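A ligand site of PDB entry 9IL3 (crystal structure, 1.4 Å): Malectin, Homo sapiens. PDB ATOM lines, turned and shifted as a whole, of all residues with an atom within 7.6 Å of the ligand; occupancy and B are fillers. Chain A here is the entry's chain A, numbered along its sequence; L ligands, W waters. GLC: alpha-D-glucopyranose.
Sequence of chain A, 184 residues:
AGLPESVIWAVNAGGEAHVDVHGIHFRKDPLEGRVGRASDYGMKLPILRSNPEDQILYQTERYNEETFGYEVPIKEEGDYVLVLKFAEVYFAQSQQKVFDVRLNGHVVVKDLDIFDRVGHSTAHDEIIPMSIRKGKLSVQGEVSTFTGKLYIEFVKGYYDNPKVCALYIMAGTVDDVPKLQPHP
The backbone NH (N) of Ser 39 sits at hydrogen-bond distance from the backbone carbonyl oxygen (O) of Glu 61 (3.1 Å). The side-chain amino group of Lys 163 lies within salt-bridge range of the side-chain carboxylate of Glu 61. The side-chain amino group of Lys 97 is in salt-bridge range of the side-chain carboxylate of Asp 160 (2.9 Å). OG of Ser 39 sits at hydrogen-bond distance from N of Tyr 41. O of Asn 161 is in hydrogen-bond range of NZ of Lys 97, at 2.9 Å. The backbone carbonyl oxygen (O) of Ala 87 sits at hydrogen-bond distance from the side-chain amino group (NZ) of Lys 163.
Water W3 lies within hydrogen-bond range of an oxygen (O1) of the ligand (2.7 Å) and the side-chain carboxylate (OD1) of Asp 160 (2.9 Å). Water W1 bridges an oxygen (O6) of the ligand (2.8 Å) and the side-chain hydroxyl of Tyr 63 (3.2 Å). Water W5 lies within hydrogen-bond range of the side-chain carboxylate of Glu 88 (2.8 Å), an oxygen (O4) of the ligand (2.9 Å), the side-chain amino group of Lys 163 (3.0 Å) and the backbone NH of Val 89 (3.0 Å).
Merely in contact with the ligand: Tyr 41, Tyr 63, Val 89 and Lys 163. Hydrophobic or aromatic side chains that line the ligand: Tyr 41, Tyr 63 and Val 89.
An oxygen (O4) of the ligand is in hydrogen-bond range of the side-chain carboxylate of Glu 61, 2.7 Å away. OD2 of Asp 160 sits at hydrogen-bond distance from O2 of the ligand, at 2.9 Å. An oxygen (O6) of the ligand lies within hydrogen-bond range of the side-chain hydroxyl of Ser 39 (2.9 Å). NZ of Lys 97 sits at hydrogen-bond distance from O3 of the ligand (2.9 Å). The side-chain amide nitrogen of Asn 161 sits at hydrogen-bond distance from an oxygen (O2) of the ligand (3.0 Å).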
ATOM      1  N   ALA A  38       1.734 -24.656  -2.211  1.00  0.00           N
ATOM      2  CA  ALA A  38       2.826 -23.692  -2.348  1.00  0.00           C
ATOM      3  C   ALA A  38       2.730 -22.966  -3.689  1.00  0.00           C
ATOM      4  O   ALA A  38       2.330 -23.556  -4.700  1.00  0.00           O
ATOM      5  CB  ALA A  38       4.172 -24.412  -2.262  1.00  0.00           C
ATOM      6  N   SER A  39       3.102 -21.674  -3.718  1.00  0.00           N
ATOM      7  CA  SER A  39       3.189 -20.920  -4.972  1.00  0.00           C
ATOM      8  C   SER A  39       4.374 -19.954  -4.966  1.00  0.00           C
ATOM      9  O   SER A  39       4.541 -19.160  -4.030  1.00  0.00           O
ATOM     10  CB  SER A  39       1.897 -20.148  -5.268  1.00  0.00           C
ATOM     11  OG  SER A  39       2.081 -19.268  -6.381  1.00  0.00           O
ATOM     12  N   ASP A  40       5.185 -20.016  -6.035  1.00  0.00           N
ATOM     13  CA  ASP A  40       6.267 -19.058  -6.282  1.00  0.00           C
ATOM     14  C   ASP A  40       5.914 -18.013  -7.360  1.00  0.00           C
ATOM     15  O   ASP A  40       6.814 -17.429  -7.977  1.00  0.00           O
ATOM     16  CB  ASP A  40       7.586 -19.768  -6.601  1.00  0.00           C
ATOM     17  CG  ASP A  40       7.519 -20.612  -7.865  1.00  0.00           C
ATOM     18  OD1 ASP A  40       6.491 -20.571  -8.568  1.00  0.00           O
ATOM     19  OD2 ASP A  40       8.510 -21.320  -8.154  1.00  0.00           O
ATOM     20  N   TYR A  41       4.615 -17.764  -7.575  1.00  0.00           N
ATOM     21  CA  TYR A  41       4.156 -16.801  -8.590  1.00  0.00           C
ATOM     22  C   TYR A  41       4.791 -15.423  -8.392  1.00  0.00           C
ATOM     23  O   TYR A  41       5.156 -14.754  -9.368  1.00  0.00           O
ATOM     24  CB  TYR A  41       2.621 -16.715  -8.582  1.00  0.00           C
ATOM     25  CG  TYR A  41       2.048 -15.770  -9.645  1.00  0.00           C
ATOM     26  CD1 TYR A  41       1.906 -16.200 -10.961  1.00  0.00           C
ATOM     27  CD2 TYR A  41       1.668 -14.459  -9.332  1.00  0.00           C
ATOM     28  CE1 TYR A  41       1.415 -15.338 -11.954  1.00  0.00           C
ATOM     29  CE2 TYR A  41       1.175 -13.599 -10.311  1.00  0.00           C
ATOM     30  CZ  TYR A  41       1.041 -14.040 -11.613  1.00  0.00           C
ATOM     31  OH  TYR A  41       0.547 -13.191 -12.600  1.00  0.00           O
ATOM     32  N   GLY A  42       4.933 -14.976  -7.146  1.00  0.00           N
ATOM     33  CA  GLY A  42       5.502 -13.658  -6.849  1.00  0.00           C
ATOM     34  C   GLY A  42       6.981 -13.479  -7.200  1.00  0.00           C
ATOM     35  O   GLY A  42       7.464 -12.332  -7.139  1.00  0.00           O
ATOM     36  N   GLU A  61       4.588 -18.246  -1.062  1.00  0.00           N
ATOM     37  CA  GLU A  61       3.425 -18.325  -0.159  1.00  0.00           C
ATOM     38  C   GLU A  61       2.924 -19.771  -0.027  1.00  0.00           C
ATOM     39  O   GLU A  61       3.228 -20.627  -0.856  1.00  0.00           O
ATOM     40  CB  GLU A  61       2.264 -17.456  -0.684  1.00  0.00           C
ATOM     41  CG  GLU A  61       1.620 -18.007  -1.986  1.00  0.00           C
ATOM     42  CD  GLU A  61       0.581 -17.062  -2.616  1.00  0.00           C
ATOM     43  OE1 GLU A  61      -0.522 -16.911  -2.035  1.00  0.00           O
ATOM     44  OE2 GLU A  61       0.887 -16.469  -3.686  1.00  0.00           O
ATOM     45  N   ARG A  62       2.104 -20.009   1.021  1.00  0.00           N
ATOM     46  CA  ARG A  62       1.179 -21.151   1.095  1.00  0.00           C
ATOM     47  C   ARG A  62      -0.253 -20.609   1.153  1.00  0.00           C
ATOM     48  O   ARG A  62      -0.535 -19.711   1.960  1.00  0.00           O
ATOM     49  CB  ARG A  62       1.453 -22.066   2.317  1.00  0.00           C
ATOM     50  CG  ARG A  62       0.631 -23.398   2.339  1.00  0.00           C
ATOM     51  CD  ARG A  62       1.242 -24.464   3.274  1.00  0.00           C
ATOM     52  NE  ARG A  62       2.523 -24.934   2.763  1.00  0.00           N
ATOM     53  CZ  ARG A  62       2.670 -25.808   1.758  1.00  0.00           C
ATOM     54  NH1 ARG A  62       1.645 -26.493   1.278  1.00  0.00           N
ATOM     55  NH2 ARG A  62       3.873 -25.967   1.213  1.00  0.00           N
ATOM     56  N   TYR A  63      -1.163 -21.149   0.308  1.00  0.00           N
ATOM     57  CA  TYR A  63      -2.578 -20.774   0.281  1.00  0.00           C
ATOM     58  C   TYR A  63      -3.469 -22.023   0.185  1.00  0.00           C
ATOM     59  O   TYR A  63      -2.972 -23.130  -0.034  1.00  0.00           O
ATOM     60  CB  TYR A  63      -2.905 -19.808  -0.872  1.00  0.00           C
ATOM     61  CG  TYR A  63      -2.992 -20.429  -2.270  1.00  0.00           C
ATOM     62  CD1 TYR A  63      -1.866 -20.580  -3.070  1.00  0.00           C
ATOM     63  CD2 TYR A  63      -4.226 -20.855  -2.794  1.00  0.00           C
ATOM     64  CE1 TYR A  63      -1.952 -21.144  -4.354  1.00  0.00           C
ATOM     65  CE2 TYR A  63      -4.307 -21.422  -4.085  1.00  0.00           C
ATOM     66  CZ  TYR A  63      -3.171 -21.562  -4.853  1.00  0.00           C
ATOM     67  OH  TYR A  63      -3.245 -22.112  -6.120  1.00  0.00           O
ATOM     68  N   ASN A  64      -4.792 -21.855   0.348  1.00  0.00           N
ATOM     69  CA  ASN A  64      -5.705 -23.015   0.264  1.00  0.00           C
ATOM     70  C   ASN A  64      -7.149 -22.540   0.056  1.00  0.00           C
ATOM     71  O   ASN A  64      -7.519 -21.445   0.458  1.00  0.00           O
ATOM     72  CB  ASN A  64      -5.607 -23.883   1.536  1.00  0.00           C
ATOM     73  CG  ASN A  64      -6.060 -25.332   1.308  1.00  0.00           C
ATOM     74  OD1 ASN A  64      -5.706 -25.957   0.314  1.00  0.00           O
ATOM     75  ND2 ASN A  64      -6.821 -25.866   2.273  1.00  0.00           N
ATOM     76  N   GLU A  65      -7.964 -23.412  -0.561  1.00  0.00           N
ATOM     77  CA  GLU A  65      -9.393 -23.134  -0.779  1.00  0.00           C
ATOM     78  C   GLU A  65     -10.262 -23.543   0.411  1.00  0.00           C
ATOM     79  O   GLU A  65     -11.487 -23.350   0.361  1.00  0.00           O
ATOM     80  CB  GLU A  65      -9.907 -23.853  -2.033  1.00  0.00           C
ATOM     81  CG  GLU A  65      -8.925 -23.909  -3.176  1.00  0.00           C
ATOM     82  CD  GLU A  65      -8.194 -25.251  -3.195  1.00  0.00           C
ATOM     83  OE1 GLU A  65      -7.088 -25.351  -2.623  1.00  0.00           O
ATOM     84  OE2 GLU A  65      -8.728 -26.202  -3.806  1.00  0.00           O
ATOM     85  N   ALA A  87       1.866 -10.467   1.445  1.00  0.00           N
ATOM     86  CA  ALA A  87       1.834  -9.599   0.263  1.00  0.00           C
ATOM     87  C   ALA A  87       0.743 -10.076  -0.697  1.00  0.00           C
ATOM     88  O   ALA A  87       0.497 -11.290  -0.800  1.00  0.00           O
ATOM     89  CB  ALA A  87       3.179  -9.537  -0.478  1.00  0.00           C
ATOM     90  N   GLU A  88       0.073  -9.125  -1.386  1.00  0.00           N
ATOM     91  CA  GLU A  88      -0.955  -9.434  -2.414  1.00  0.00           C
ATOM     92  C   GLU A  88      -0.308  -9.359  -3.797  1.00  0.00           C
ATOM     93  O   GLU A  88      -0.064  -8.264  -4.322  1.00  0.00           O
ATOM     94  CB  GLU A  88      -2.153  -8.494  -2.301  1.00  0.00           C
ATOM     95  CG  GLU A  88      -3.246  -8.682  -3.392  1.00  0.00           C
ATOM     96  CD  GLU A  88      -3.816 -10.106  -3.427  1.00  0.00           C
ATOM     97  OE1 GLU A  88      -4.603 -10.459  -2.514  1.00  0.00           O
ATOM     98  OE2 GLU A  88      -3.467 -10.883  -4.356  1.00  0.00           O
ATOM     99  N   VAL A  89      -0.023 -10.521  -4.398  1.00  0.00           N
ATOM    100  CA  VAL A  89       0.713 -10.601  -5.673  1.00  0.00           C
ATOM    101  C   VAL A  89      -0.194 -10.860  -6.880  1.00  0.00           C
ATOM    102  O   VAL A  89       0.311 -11.092  -7.996  1.00  0.00           O
ATOM    103  CB  VAL A  89       1.914 -11.599  -5.613  1.00  0.00           C
ATOM    104  CG1 VAL A  89       2.942 -11.176  -4.524  1.00  0.00           C
ATOM    105  CG2 VAL A  89       1.413 -13.028  -5.371  1.00  0.00           C
ATOM    106  N   TYR A  90      -1.532 -10.826  -6.689  1.00  0.00           N
ATOM    107  CA  TYR A  90      -2.500 -11.127  -7.758  1.00  0.00           C
ATOM    108  C   TYR A  90      -3.523 -10.011  -7.975  1.00  0.00           C
ATOM    109  O   TYR A  90      -3.626  -9.460  -9.090  1.00  0.00           O
ATOM    110  CB  TYR A  90      -3.163 -12.511  -7.573  1.00  0.00           C
ATOM    111  CG  TYR A  90      -3.924 -13.036  -8.804  1.00  0.00           C
ATOM    112  CD1 TYR A  90      -3.250 -13.549  -9.913  1.00  0.00           C
ATOM    113  CD2 TYR A  90      -5.317 -13.002  -8.858  1.00  0.00           C
ATOM    114  CE1 TYR A  90      -3.952 -14.028 -11.044  1.00  0.00           C
ATOM    115  CE2 TYR A  90      -6.028 -13.489  -9.977  1.00  0.00           C
ATOM    116  CZ  TYR A  90      -5.338 -13.984 -11.053  1.00  0.00           C
ATOM    117  OH  TYR A  90      -6.050 -14.442 -12.163  1.00  0.00           O
ATOM    118  N   PHE A  91      -4.280  -9.627  -6.934  1.00  0.00           N
ATOM    119  CA  PHE A  91      -5.372  -8.653  -7.045  1.00  0.00           C
ATOM    120  C   PHE A  91      -4.889  -7.208  -6.864  1.00  0.00           C
ATOM    121  O   PHE A  91      -3.811  -6.936  -6.305  1.00  0.00           O
ATOM    122  CB  PHE A  91      -6.495  -8.967  -6.043  1.00  0.00           C
ATOM    123  CG  PHE A  91      -7.190 -10.288  -6.287  1.00  0.00           C
ATOM    124  CD1 PHE A  91      -8.095 -10.426  -7.347  1.00  0.00           C
ATOM    125  CD2 PHE A  91      -6.967 -11.388  -5.456  1.00  0.00           C
ATOM    126  CE1 PHE A  91      -8.757 -11.643  -7.570  1.00  0.00           C
ATOM    127  CE2 PHE A  91      -7.625 -12.611  -5.672  1.00  0.00           C
ATOM    128  CZ  PHE A  91      -8.515 -12.733  -6.742  1.00  0.00           C
ATOM    129  N   LYS A  97      -9.810 -10.423  -1.989  1.00  0.00           N
ATOM    130  CA  LYS A  97      -9.327 -11.458  -1.070  1.00  0.00           C
ATOM    131  C   LYS A  97      -9.418 -10.943   0.370  1.00  0.00           C
ATOM    132  O   LYS A  97      -8.785  -9.920   0.693  1.00  0.00           O
ATOM    133  CB  LYS A  97      -7.876 -11.868  -1.407  1.00  0.00           C
ATOM    134  CG  LYS A  97      -7.269 -12.936  -0.444  1.00  0.00           C
ATOM    135  CD  LYS A  97      -5.714 -13.055  -0.517  1.00  0.00           C
ATOM    136  CE  LYS A  97      -5.187 -13.647  -1.827  1.00  0.00           C
ATOM    137  NZ  LYS A  97      -5.522 -15.114  -1.995  1.00  0.00           N
ATOM    138  N   ASP A 160     -12.155 -15.097  -2.195  1.00  0.00           N
ATOM    139  CA  ASP A 160     -10.894 -15.788  -2.536  1.00  0.00           C
ATOM    140  C   ASP A 160     -10.351 -16.627  -1.374  1.00  0.00           C
ATOM    141  O   ASP A 160     -11.119 -17.074  -0.503  1.00  0.00           O
ATOM    142  CB  ASP A 160      -9.869 -14.850  -3.181  1.00  0.00           C
ATOM    143  CG  ASP A 160      -8.946 -15.567  -4.170  1.00  0.00           C
ATOM    144  OD1 ASP A 160      -9.412 -16.114  -5.208  1.00  0.00           O
ATOM    145  OD2 ASP A 160      -7.730 -15.702  -3.850  1.00  0.00           O
ATOM    146  N   ASN A 161      -9.012 -16.835  -1.315  1.00  0.00           N
ATOM    147  CA  ASN A 161      -8.380 -17.867  -0.489  1.00  0.00           C
ATOM    148  C   ASN A 161      -7.468 -17.288   0.604  1.00  0.00           C
ATOM    149  O   ASN A 161      -6.702 -16.357   0.343  1.00  0.00           O
ATOM    150  CB  ASN A 161      -7.541 -18.822  -1.383  1.00  0.00           C
ATOM    151  CG  ASN A 161      -8.350 -19.468  -2.502  1.00  0.00           C
ATOM    152  OD1 ASN A 161      -9.473 -19.938  -2.282  1.00  0.00           O
ATOM    153  ND2 ASN A 161      -7.767 -19.546  -3.693  1.00  0.00           N
ATOM    154  N   PRO A 162      -7.505 -17.855   1.825  1.00  0.00           N
ATOM    155  CA  PRO A 162      -6.516 -17.465   2.855  1.00  0.00           C
ATOM    156  C   PRO A 162      -5.082 -17.825   2.441  1.00  0.00           C
ATOM    157  O   PRO A 162      -4.854 -18.802   1.712  1.00  0.00           O
ATOM    158  CB  PRO A 162      -6.937 -18.283   4.090  1.00  0.00           C
ATOM    159  CG  PRO A 162      -7.746 -19.447   3.533  1.00  0.00           C
ATOM    160  CD  PRO A 162      -8.451 -18.862   2.318  1.00  0.00           C
ATOM    161  N   LYS A 163      -4.109 -17.033   2.924  1.00  0.00           N
ATOM    162  CA  LYS A 163      -2.690 -17.225   2.580  1.00  0.00           C
ATOM    163  C   LYS A 163      -1.768 -16.668   3.666  1.00  0.00           C
ATOM    164  O   LYS A 163      -2.191 -15.869   4.514  1.00  0.00           O
ATOM    165  CB  LYS A 163      -2.355 -16.549   1.227  1.00  0.00           C
ATOM    166  CG  LYS A 163      -2.298 -14.996   1.282  1.00  0.00           C
ATOM    167  CD  LYS A 163      -1.811 -14.377  -0.046  1.00  0.00           C
ATOM    168  CE  LYS A 163      -0.274 -14.336  -0.121  1.00  0.00           C
ATOM    169  NZ  LYS A 163       0.201 -14.003  -1.513  1.00  0.00           N
ATOM    170  N   VAL A 164      -0.493 -17.087   3.624  1.00  0.00           N
ATOM    171  CA  VAL A 164       0.576 -16.517   4.460  1.00  0.00           C
ATOM    172  C   VAL A 164       1.928 -16.638   3.739  1.00  0.00           C
ATOM    173  O   VAL A 164       2.158 -17.596   2.984  1.00  0.00           O
ATOM    174  CB  VAL A 164       0.611 -17.148   5.894  1.00  0.00           C
ATOM    175  CG1 VAL A 164       1.041 -18.614   5.847  1.00  0.00           C
ATOM    176  CG2 VAL A 164       1.508 -16.324   6.856  1.00  0.00           C
HETATM  177  C1  GLC L   1      -4.481 -17.792  -6.302  1.00  0.00           C
HETATM  178  C2  GLC L   1      -4.251 -17.626  -4.839  1.00  0.00           C
HETATM  179  C3  GLC L   1      -3.372 -16.478  -4.568  1.00  0.00           C
HETATM  180  C4  GLC L   1      -2.067 -16.578  -5.301  1.00  0.00           C
HETATM  181  C5  GLC L   1      -2.260 -16.721  -6.835  1.00  0.00           C
HETATM  182  C6  GLC L   1      -1.024 -16.918  -7.537  1.00  0.00           C
HETATM  183  O1  GLC L   1      -5.180 -16.677  -6.780  1.00  0.00           O
HETATM  184  O2  GLC L   1      -5.560 -17.532  -4.121  1.00  0.00           O
HETATM  185  O3  GLC L   1      -3.107 -16.358  -3.117  1.00  0.00           O
HETATM  186  O4  GLC L   1      -1.243 -15.427  -5.052  1.00  0.00           O
HETATM  187  O5  GLC L   1      -3.200 -17.914  -7.026  1.00  0.00           O
HETATM  188  O6  GLC L   1      -0.431 -18.169  -7.246  1.00  0.00           O
HETATM  189  O   HOH W   1      -1.472 -20.604  -8.260  1.00  0.00           O
HETATM  190  O   HOH W   2      -6.366 -17.583  -9.795  1.00  0.00           O
HETATM  191  O   HOH W   3      -7.753 -17.165  -7.366  1.00  0.00           O
HETATM  192  O   HOH W   4      -3.722 -18.545  -9.874  1.00  0.00           O
HETATM  193  O   HOH W   5      -1.679 -12.913  -3.584  1.00  0.00           O
